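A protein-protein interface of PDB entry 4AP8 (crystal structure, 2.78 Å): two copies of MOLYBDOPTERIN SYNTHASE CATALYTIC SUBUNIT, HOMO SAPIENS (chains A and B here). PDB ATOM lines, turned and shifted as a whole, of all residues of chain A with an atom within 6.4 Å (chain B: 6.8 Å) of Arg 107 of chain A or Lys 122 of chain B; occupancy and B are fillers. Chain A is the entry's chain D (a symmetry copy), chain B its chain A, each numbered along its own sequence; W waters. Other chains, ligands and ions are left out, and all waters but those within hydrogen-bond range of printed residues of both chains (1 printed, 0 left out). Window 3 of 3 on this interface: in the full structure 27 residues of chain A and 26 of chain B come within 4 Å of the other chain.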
ATOM      1  N   GLY A  32       8.827  -9.293  22.971  1.00  0.00           N
ATOM      2  CA  GLY A  32      10.014  -9.233  22.135  1.00  0.00           C
ATOM      3  C   GLY A  32      11.301  -9.737  22.782  1.00  0.00           C
ATOM      4  O   GLY A  32      12.343  -9.837  22.093  1.00  0.00           O
ATOM      5  N   ALA A  33      11.250 -10.053  24.081  1.00  0.00           N
ATOM      6  CA  ALA A  33      12.458 -10.500  24.809  1.00  0.00           C
ATOM      7  C   ALA A  33      12.140 -11.660  25.698  1.00  0.00           C
ATOM      8  O   ALA A  33      11.090 -11.693  26.322  1.00  0.00           O
ATOM      9  CB  ALA A  33      13.031  -9.388  25.670  1.00  0.00           C
ATOM     10  N   ILE A  34      13.049 -12.610  25.738  1.00  0.00           N
ATOM     11  CA  ILE A  34      13.024 -13.664  26.710  1.00  0.00           C
ATOM     12  C   ILE A  34      14.424 -13.773  27.244  1.00  0.00           C
ATOM     13  O   ILE A  34      15.371 -13.908  26.460  1.00  0.00           O
ATOM     14  CB  ILE A  34      12.726 -15.007  26.079  1.00  0.00           C
ATOM     15  CG1 ILE A  34      11.358 -15.010  25.462  1.00  0.00           C
ATOM     16  CG2 ILE A  34      12.811 -16.094  27.136  1.00  0.00           C
ATOM     17  CD1 ILE A  34      11.095 -16.334  24.792  1.00  0.00           C
ATOM     18  N   SER A  35      14.568 -13.733  28.552  1.00  0.00           N
ATOM     19  CA  SER A  35      15.873 -13.950  29.150  1.00  0.00           C
ATOM     20  C   SER A  35      15.819 -15.265  29.875  1.00  0.00           C
ATOM     21  O   SER A  35      14.781 -15.636  30.392  1.00  0.00           O
ATOM     22  CB  SER A  35      16.219 -12.811  30.097  1.00  0.00           C
ATOM     23  OG  SER A  35      16.483 -11.613  29.392  1.00  0.00           O
ATOM     24  N   SER A 104       9.053 -10.472  28.119  1.00  0.00           N
ATOM     25  CA  SER A 104       8.534  -9.103  28.216  1.00  0.00           C
ATOM     26  C   SER A 104       8.555  -8.423  26.882  1.00  0.00           C
ATOM     27  O   SER A 104       9.156  -8.929  25.920  1.00  0.00           O
ATOM     28  CB  SER A 104       9.364  -8.277  29.187  1.00  0.00           C
ATOM     29  OG  SER A 104      10.731  -8.297  28.802  1.00  0.00           O
ATOM     30  N   ALA A 105       7.901  -7.267  26.847  1.00  0.00           N
ATOM     31  CA  ALA A 105       7.842  -6.435  25.654  1.00  0.00           C
ATOM     32  C   ALA A 105       9.252  -6.088  25.230  1.00  0.00           C
ATOM     33  O   ALA A 105       9.644  -6.308  24.074  1.00  0.00           O
ATOM     34  CB  ALA A 105       7.079  -5.157  25.950  1.00  0.00           C
ATOM     35  N   HIS A 106      10.016  -5.581  26.198  1.00  0.00           N
ATOM     36  CA  HIS A 106      11.351  -5.082  25.943  1.00  0.00           C
ATOM     37  C   HIS A 106      12.368  -5.723  26.817  1.00  0.00           C
ATOM     38  O   HIS A 106      12.061  -6.212  27.900  1.00  0.00           O
ATOM     39  CB  HIS A 106      11.357  -3.583  26.106  1.00  0.00           C
ATOM     40  CG  HIS A 106      10.344  -2.898  25.251  1.00  0.00           C
ATOM     41  ND1 HIS A 106      10.402  -2.921  23.907  1.00  0.00           N
ATOM     42  CD2 HIS A 106       9.209  -2.168  25.586  1.00  0.00           C
ATOM     43  CE1 HIS A 106       9.366  -2.229  23.402  1.00  0.00           C
ATOM     44  NE2 HIS A 106       8.639  -1.760  24.433  1.00  0.00           N
ATOM     45  N   ARG A 107      13.615  -5.716  26.367  1.00  0.00           N
ATOM     46  CA  ARG A 107      14.619  -6.564  27.002  1.00  0.00           C
ATOM     47  C   ARG A 107      14.987  -6.218  28.429  1.00  0.00           C
ATOM     48  O   ARG A 107      15.172  -7.114  29.256  1.00  0.00           O
ATOM     49  CB  ARG A 107      15.859  -6.622  26.165  1.00  0.00           C
ATOM     50  CG  ARG A 107      16.535  -5.307  25.892  1.00  0.00           C
ATOM     51  CD  ARG A 107      17.883  -5.575  25.216  1.00  0.00           C
ATOM     52  NE  ARG A 107      18.595  -4.347  24.913  1.00  0.00           N
ATOM     53  CZ  ARG A 107      18.252  -3.493  23.968  1.00  0.00           C
ATOM     54  NH1 ARG A 107      17.234  -3.751  23.149  1.00  0.00           N
ATOM     55  NH2 ARG A 107      18.970  -2.392  23.817  1.00  0.00           N
ATOM     56  N   ALA A 108      15.037  -4.930  28.742  1.00  0.00           N
ATOM     57  CA  ALA A 108      15.407  -4.495  30.090  1.00  0.00           C
ATOM     58  C   ALA A 108      14.650  -5.248  31.190  1.00  0.00           C
ATOM     59  O   ALA A 108      15.278  -5.791  32.103  1.00  0.00           O
ATOM     60  CB  ALA A 108      15.219  -3.011  30.241  1.00  0.00           C
ATOM     61  N   ALA A 109      13.328  -5.315  31.072  1.00  0.00           N
ATOM     62  CA  ALA A 109      12.532  -5.992  32.065  1.00  0.00           C
ATOM     63  C   ALA A 109      12.984  -7.447  32.200  1.00  0.00           C
ATOM     64  O   ALA A 109      13.298  -7.921  33.304  1.00  0.00           O
ATOM     65  CB  ALA A 109      11.073  -5.916  31.706  1.00  0.00           C
ATOM     66  N   SER A 110      13.082  -8.153  31.086  1.00  0.00           N
ATOM     67  CA  SER A 110      13.385  -9.561  31.196  1.00  0.00           C
ATOM     68  C   SER A 110      14.808  -9.771  31.745  1.00  0.00           C
ATOM     69  O   SER A 110      15.049 -10.650  32.568  1.00  0.00           O
ATOM     70  CB  SER A 110      13.205 -10.269  29.863  1.00  0.00           C
ATOM     71  OG  SER A 110      14.241  -9.934  28.977  1.00  0.00           O
ATOM     72  N   LEU A 111      15.742  -8.942  31.327  1.00  0.00           N
ATOM     73  CA  LEU A 111      17.102  -9.104  31.795  1.00  0.00           C
ATOM     74  C   LEU A 111      17.177  -8.868  33.316  1.00  0.00           C
ATOM     75  O   LEU A 111      17.719  -9.684  34.058  1.00  0.00           O
ATOM     76  CB  LEU A 111      18.042  -8.145  31.043  1.00  0.00           C
ATOM     77  CG  LEU A 111      18.289  -8.531  29.595  1.00  0.00           C
ATOM     78  CD1 LEU A 111      18.796  -7.344  28.789  1.00  0.00           C
ATOM     79  CD2 LEU A 111      19.244  -9.702  29.572  1.00  0.00           C
ATOM     80  N   GLU A 112      16.669  -7.731  33.749  1.00  0.00           N
ATOM     81  CA  GLU A 112      16.716  -7.372  35.142  1.00  0.00           C
ATOM     82  C   GLU A 112      15.936  -8.386  35.948  1.00  0.00           C
ATOM     83  O   GLU A 112      16.430  -8.845  36.981  1.00  0.00           O
ATOM     84  CB  GLU A 112      16.195  -5.947  35.364  1.00  0.00           C
ATOM     85  CG  GLU A 112      17.276  -4.866  35.245  1.00  0.00           C
ATOM     86  CD  GLU A 112      16.755  -3.523  34.739  1.00  0.00           C
ATOM     87  OE1 GLU A 112      15.742  -3.041  35.261  1.00  0.00           O
ATOM     88  OE2 GLU A 112      17.334  -2.950  33.785  1.00  0.00           O
ATOM     89  N   PHE B  37      19.847 -14.789  26.052  1.00  0.00           N
ATOM     90  CA  PHE B  37      18.849 -13.839  25.657  1.00  0.00           C
ATOM     91  C   PHE B  37      18.306 -14.243  24.335  1.00  0.00           C
ATOM     92  O   PHE B  37      19.084 -14.560  23.454  1.00  0.00           O
ATOM     93  CB  PHE B  37      19.442 -12.492  25.492  1.00  0.00           C
ATOM     94  CG  PHE B  37      18.464 -11.493  25.049  1.00  0.00           C
ATOM     95  CD1 PHE B  37      17.614 -10.926  25.955  1.00  0.00           C
ATOM     96  CD2 PHE B  37      18.373 -11.144  23.737  1.00  0.00           C
ATOM     97  CE1 PHE B  37      16.665 -10.011  25.558  1.00  0.00           C
ATOM     98  CE2 PHE B  37      17.447 -10.231  23.328  1.00  0.00           C
ATOM     99  CZ  PHE B  37      16.582  -9.660  24.244  1.00  0.00           C
ATOM    100  N   GLY B  39      15.716 -12.798  21.365  1.00  0.00           N
ATOM    101  CA  GLY B  39      14.959 -11.689  20.776  1.00  0.00           C
ATOM    102  C   GLY B  39      13.912 -12.200  19.815  1.00  0.00           C
ATOM    103  O   GLY B  39      14.217 -12.974  18.935  1.00  0.00           O
ATOM    104  N   TYR B  55      15.281  -8.375   8.641  1.00  0.00           N
ATOM    105  CA  TYR B  55      16.594  -7.957   9.096  1.00  0.00           C
ATOM    106  C   TYR B  55      17.614  -8.086   7.956  1.00  0.00           C
ATOM    107  O   TYR B  55      17.642  -9.100   7.242  1.00  0.00           O
ATOM    108  CB  TYR B  55      17.018  -8.831  10.245  1.00  0.00           C
ATOM    109  CG  TYR B  55      16.234  -8.575  11.498  1.00  0.00           C
ATOM    110  CD1 TYR B  55      16.626  -7.613  12.385  1.00  0.00           C
ATOM    111  CD2 TYR B  55      15.106  -9.301  11.801  1.00  0.00           C
ATOM    112  CE1 TYR B  55      15.908  -7.374  13.544  1.00  0.00           C
ATOM    113  CE2 TYR B  55      14.386  -9.081  12.974  1.00  0.00           C
ATOM    114  CZ  TYR B  55      14.778  -8.116  13.830  1.00  0.00           C
ATOM    115  OH  TYR B  55      14.075  -7.885  14.993  1.00  0.00           O
ATOM    116  N   ILE B  69      32.747  -7.375  20.384  1.00  0.00           N
ATOM    117  CA  ILE B  69      31.998  -7.522  21.591  1.00  0.00           C
ATOM    118  C   ILE B  69      32.533  -8.698  22.388  1.00  0.00           C
ATOM    119  O   ILE B  69      32.711  -8.607  23.586  1.00  0.00           O
ATOM    120  CB  ILE B  69      30.515  -7.733  21.325  1.00  0.00           C
ATOM    121  CG1 ILE B  69      29.896  -6.439  20.773  1.00  0.00           C
ATOM    122  CG2 ILE B  69      29.881  -8.187  22.644  1.00  0.00           C
ATOM    123  CD1 ILE B  69      28.429  -6.526  20.415  1.00  0.00           C
ATOM    124  N   HIS B  86      22.254 -14.503  14.916  1.00  0.00           N
ATOM    125  CA  HIS B  86      21.279 -13.540  14.424  1.00  0.00           C
ATOM    126  C   HIS B  86      20.670 -14.052  13.166  1.00  0.00           C
ATOM    127  O   HIS B  86      21.366 -14.611  12.294  1.00  0.00           O
ATOM    128  CB  HIS B  86      21.932 -12.196  14.157  1.00  0.00           C
ATOM    129  CG  HIS B  86      20.985 -11.060  14.222  1.00  0.00           C
ATOM    130  ND1 HIS B  86      19.844 -11.032  13.508  1.00  0.00           N
ATOM    131  CD2 HIS B  86      21.008  -9.900  14.990  1.00  0.00           C
ATOM    132  CE1 HIS B  86      19.171  -9.897  13.802  1.00  0.00           C
ATOM    133  NE2 HIS B  86      19.880  -9.209  14.706  1.00  0.00           N
ATOM    134  N   SER B  97      14.762 -13.714  16.373  1.00  0.00           N
ATOM    135  CA  SER B  97      15.719 -13.000  15.526  1.00  0.00           C
ATOM    136  C   SER B  97      17.140 -13.029  16.097  1.00  0.00           C
ATOM    137  O   SER B  97      18.112 -12.911  15.356  1.00  0.00           O
ATOM    138  CB  SER B  97      15.284 -11.543  15.342  1.00  0.00           C
ATOM    139  OG  SER B  97      15.130 -10.906  16.587  1.00  0.00           O
ATOM    140  N   ILE B  98      17.274 -13.143  17.410  1.00  0.00           N
ATOM    141  CA  ILE B  98      18.591 -13.202  17.991  1.00  0.00           C
ATOM    142  C   ILE B  98      18.575 -14.115  19.203  1.00  0.00           C
ATOM    143  O   ILE B  98      17.637 -14.093  19.968  1.00  0.00           O
ATOM    144  CB  ILE B  98      19.197 -11.797  18.276  1.00  0.00           C
ATOM    145  CG1 ILE B  98      20.453 -11.938  19.100  1.00  0.00           C
ATOM    146  CG2 ILE B  98      18.269 -10.820  18.911  1.00  0.00           C
ATOM    147  CD1 ILE B  98      21.172 -10.620  19.216  1.00  0.00           C
ATOM    148  N   SER B 115      23.826  -9.395  29.193  1.00  0.00           N
ATOM    149  CA  SER B 115      23.157  -8.079  29.066  1.00  0.00           C
ATOM    150  C   SER B 115      24.070  -7.151  28.296  1.00  0.00           C
ATOM    151  O   SER B 115      23.595  -6.392  27.523  1.00  0.00           O
ATOM    152  CB  SER B 115      22.787  -7.374  30.367  1.00  0.00           C
ATOM    153  OG  SER B 115      23.975  -7.209  31.057  1.00  0.00           O
ATOM    154  N   TYR B 116      25.364  -7.151  28.592  1.00  0.00           N
ATOM    155  CA  TYR B 116      26.258  -6.225  27.942  1.00  0.00           C
ATOM    156  C   TYR B 116      26.227  -6.539  26.456  1.00  0.00           C
ATOM    157  O   TYR B 116      26.177  -5.645  25.611  1.00  0.00           O
ATOM    158  CB  TYR B 116      27.684  -6.345  28.498  1.00  0.00           C
ATOM    159  CG  TYR B 116      28.686  -5.628  27.655  1.00  0.00           C
ATOM    160  CD1 TYR B 116      28.897  -4.282  27.804  1.00  0.00           C
ATOM    161  CD2 TYR B 116      29.374  -6.277  26.669  1.00  0.00           C
ATOM    162  CE1 TYR B 116      29.796  -3.610  27.011  1.00  0.00           C
ATOM    163  CE2 TYR B 116      30.255  -5.601  25.861  1.00  0.00           C
ATOM    164  CZ  TYR B 116      30.475  -4.272  26.039  1.00  0.00           C
ATOM    165  OH  TYR B 116      31.388  -3.603  25.241  1.00  0.00           O
ATOM    166  N   ALA B 117      26.244  -7.828  26.149  1.00  0.00           N
ATOM    167  CA  ALA B 117      26.275  -8.297  24.765  1.00  0.00           C
ATOM    168  C   ALA B 117      25.063  -7.822  23.955  1.00  0.00           C
ATOM    169  O   ALA B 117      25.220  -7.255  22.889  1.00  0.00           O
ATOM    170  CB  ALA B 117      26.383  -9.806  24.736  1.00  0.00           C
ATOM    171  N   ILE B 118      23.869  -7.973  24.509  1.00  0.00           N
ATOM    172  CA  ILE B 118      22.668  -7.595  23.784  1.00  0.00           C
ATOM    173  C   ILE B 118      22.596  -6.077  23.661  1.00  0.00           C
ATOM    174  O   ILE B 118      22.291  -5.577  22.582  1.00  0.00           O
ATOM    175  CB  ILE B 118      21.368  -8.205  24.372  1.00  0.00           C
ATOM    176  CG1 ILE B 118      20.150  -7.857  23.527  1.00  0.00           C
ATOM    177  CG2 ILE B 118      21.107  -7.723  25.761  1.00  0.00           C
ATOM    178  CD1 ILE B 118      20.300  -8.250  22.072  1.00  0.00           C
ATOM    179  N   ASP B 119      22.926  -5.340  24.715  1.00  0.00           N
ATOM    180  CA  ASP B 119      22.828  -3.882  24.619  1.00  0.00           C
ATOM    181  C   ASP B 119      23.853  -3.417  23.615  1.00  0.00           C
ATOM    182  O   ASP B 119      23.567  -2.586  22.766  1.00  0.00           O
ATOM    183  CB  ASP B 119      23.066  -3.166  25.938  1.00  0.00           C
ATOM    184  CG  ASP B 119      21.964  -3.423  26.965  1.00  0.00           C
ATOM    185  OD1 ASP B 119      20.800  -3.591  26.547  1.00  0.00           O
ATOM    186  OD2 ASP B 119      22.259  -3.409  28.196  1.00  0.00           O
ATOM    187  N   THR B 120      25.038  -3.989  23.672  1.00  0.00           N
ATOM    188  CA  THR B 120      26.084  -3.493  22.826  1.00  0.00           C
ATOM    189  C   THR B 120      25.818  -3.857  21.366  1.00  0.00           C
ATOM    190  O   THR B 120      26.083  -3.074  20.448  1.00  0.00           O
ATOM    191  CB  THR B 120      27.458  -3.983  23.289  1.00  0.00           C
ATOM    192  OG1 THR B 120      27.746  -3.432  24.577  1.00  0.00           O
ATOM    193  CG2 THR B 120      28.546  -3.529  22.311  1.00  0.00           C
ATOM    194  N   LEU B 121      25.278  -5.035  21.136  1.00  0.00           N
ATOM    195  CA  LEU B 121      24.971  -5.445  19.774  1.00  0.00           C
ATOM    196  C   LEU B 121      23.934  -4.491  19.179  1.00  0.00           C
ATOM    197  O   LEU B 121      24.059  -4.061  18.062  1.00  0.00           O
ATOM    198  CB  LEU B 121      24.473  -6.894  19.746  1.00  0.00           C
ATOM    199  CG  LEU B 121      23.968  -7.440  18.401  1.00  0.00           C
ATOM    200  CD1 LEU B 121      23.935  -8.959  18.364  1.00  0.00           C
ATOM    201  CD2 LEU B 121      22.558  -6.928  18.168  1.00  0.00           C
ATOM    202  N   LYS B 122      22.891  -4.180  19.927  1.00  0.00           N
ATOM    203  CA  LYS B 122      21.886  -3.254  19.428  1.00  0.00           C
ATOM    204  C   LYS B 122      22.503  -1.880  19.198  1.00  0.00           C
ATOM    205  O   LYS B 122      22.073  -1.146  18.345  1.00  0.00           O
ATOM    206  CB  LYS B 122      20.697  -3.133  20.390  1.00  0.00           C
ATOM    207  CG  LYS B 122      19.780  -4.360  20.548  1.00  0.00           C
ATOM    208  CD  LYS B 122      19.192  -4.901  19.242  1.00  0.00           C
ATOM    209  CE  LYS B 122      17.700  -5.275  19.347  1.00  0.00           C
ATOM    210  NZ  LYS B 122      17.269  -6.280  18.332  1.00  0.00           N
ATOM    211  N   ALA B 123      23.510  -1.514  19.956  1.00  0.00           N
ATOM    212  CA  ALA B 123      24.093  -0.194  19.774  1.00  0.00           C
ATOM    213  C   ALA B 123      25.057  -0.137  18.611  1.00  0.00           C
ATOM    214  O   ALA B 123      25.118   0.860  17.975  1.00  0.00           O
ATOM    215  CB  ALA B 123      24.830   0.252  21.021  1.00  0.00           C
ATOM    216  N   LYS B 124      25.849  -1.170  18.389  1.00  0.00           N
ATOM    217  CA  LYS B 124      27.047  -1.018  17.578  1.00  0.00           C
ATOM    218  C   LYS B 124      27.073  -1.866  16.308  1.00  0.00           C
ATOM    219  O   LYS B 124      27.889  -1.612  15.442  1.00  0.00           O
ATOM    220  CB  LYS B 124      28.330  -1.225  18.449  1.00  0.00           C
ATOM    221  CG  LYS B 124      28.673  -0.009  19.321  1.00  0.00           C
ATOM    222  CD  LYS B 124      29.655   1.034  18.681  1.00  0.00           C
ATOM    223  N   VAL B 125      26.177  -2.829  16.153  1.00  0.00           N
ATOM    224  CA  VAL B 125      26.253  -3.755  15.019  1.00  0.00           C
ATOM    225  C   VAL B 125      25.308  -3.363  13.879  1.00  0.00           C
ATOM    226  O   VAL B 125      24.136  -3.252  14.077  1.00  0.00           O
ATOM    227  CB  VAL B 125      25.923  -5.200  15.438  1.00  0.00           C
ATOM    228  CG1 VAL B 125      26.086  -6.172  14.263  1.00  0.00           C
ATOM    229  CG2 VAL B 125      26.851  -5.624  16.533  1.00  0.00           C
ATOM    230  N   LYS B 129      16.535  -3.118  10.536  1.00  0.00           N
ATOM    231  CA  LYS B 129      15.244  -3.821  10.642  1.00  0.00           C
ATOM    232  C   LYS B 129      14.138  -2.987  10.034  1.00  0.00           C
ATOM    233  O   LYS B 129      14.112  -1.794  10.263  1.00  0.00           O
ATOM    234  CB  LYS B 129      14.872  -4.247  12.072  1.00  0.00           C
ATOM    235  CG  LYS B 129      14.183  -3.215  12.965  1.00  0.00           C
ATOM    236  CD  LYS B 129      13.697  -3.867  14.264  1.00  0.00           C
ATOM    237  CE  LYS B 129      13.674  -2.919  15.464  1.00  0.00           C
ATOM    238  NZ  LYS B 129      12.699  -1.806  15.375  1.00  0.00           N
HETATM  239  O   HOH W   1      18.614  -3.687  28.234  1.00  0.00           O
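No position is printed for both chains.
Of the 9 pairs that touch across the chains among the printed residues, none has its exchanged pair printed and touching as well.
Of chain A, only Arg 107 (3.7 Å) comes within 4 Å of Lys 122 of chain B.
Of the printed residues of chain A, Ile 118 of chain B touches Arg 107 and Leu 111.
Printed residues of chain A within 4 Å of Asp 119 of chain B: Arg 107 (2.8 Å).
Of the printed residues of chain B, Ala 33 of chain A touches Phe 37 (3.7 Å).
Printed residues of chain A within 4 Å of Phe 37 of chain B: Ala 33 (3.7 Å), Ile 34 (3.6 Å), Ser 35 (3.7 Å) and Arg 107 (3.5 Å).
Of the printed residues of chain B, Ser 35 of chain A touches Phe 37.
Ala 123 of chain B touches none of the printed residues of chain A.
Glu 112 of chain A touches none of the printed residues of chain B.
Water W1 lies within hydrogen-bond range of the side-chain carboxylate of Asp 119 of chain B (2.8 Å) and the guanidinium group of Arg 107 of chain A (3.4 Å).
Among the printed residues, merely in contact across the chains: Gly 32 of chain A with Gly 39 of chain B, Ala 33 of chain A with Phe 37 of chain B, Ile 34 of chain A with Phe 37 of chain B, Ser 35 of chain A with Phe 37 of chain B, Arg 107 of chain A with Phe 37 of chain B, Arg 107 of chain A with Ile 118 of chain B, Arg 107 of chain A with Lys 122 of chain B and Leu 111 of chain A with Ile 118 of chain B.
The backbone carbonyl oxygen of Ser 104 of chain A is in hydrogen-bond range of the backbone NH of Gly 32 of chain A (3.0 Å).
The backbone NH (N) of Ser 97 of chain B is in hydrogen-bond range of the backbone carbonyl oxygen (O) of Gly 39 of chain B, 2.7 Å away.
The backbone NH of Leu 111 of chain A lies close to the side-chain hydroxyl of Ser 35 of chain A.
The side-chain hydroxyl (OG) of Ser 35 of chain A lies within hydrogen-bond range of the side-chain hydroxyl (OG) of Ser 110 of chain A, 2.8 Å away.
N of Gly 39 of chain B sits at hydrogen-bond distance from O of Ile 98 of chain B, 2.7 Å away.
OG of Ser 110 of chain A sits at hydrogen-bond distance from O of Arg 107 of chain A, at 3.0 Å.
Of the 13 printed residues of chain A, 6 touch a printed residue of chain B.
Hydrophobic or aromatic side chains of chain A that line the printed part of chain B: Ala 33 and Leu 111.
Of the 19 printed residues of chain B, 5 touch a printed residue of chain A.
Among the printed residues, 9 pairs touch across the chains.
Among the printed residues, Asp or Glu carboxylates within 4 Å of a Lys or Arg side-chain nitrogen of the other chain: Arg 107 of chain A with Asp 119 of chain B (2.8 Å).
The guanidinium group (NE) of Arg 107 of chain A is in salt-bridge range of the side-chain carboxylate (OD1) of Asp 119 of chain B (2.8 Å).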
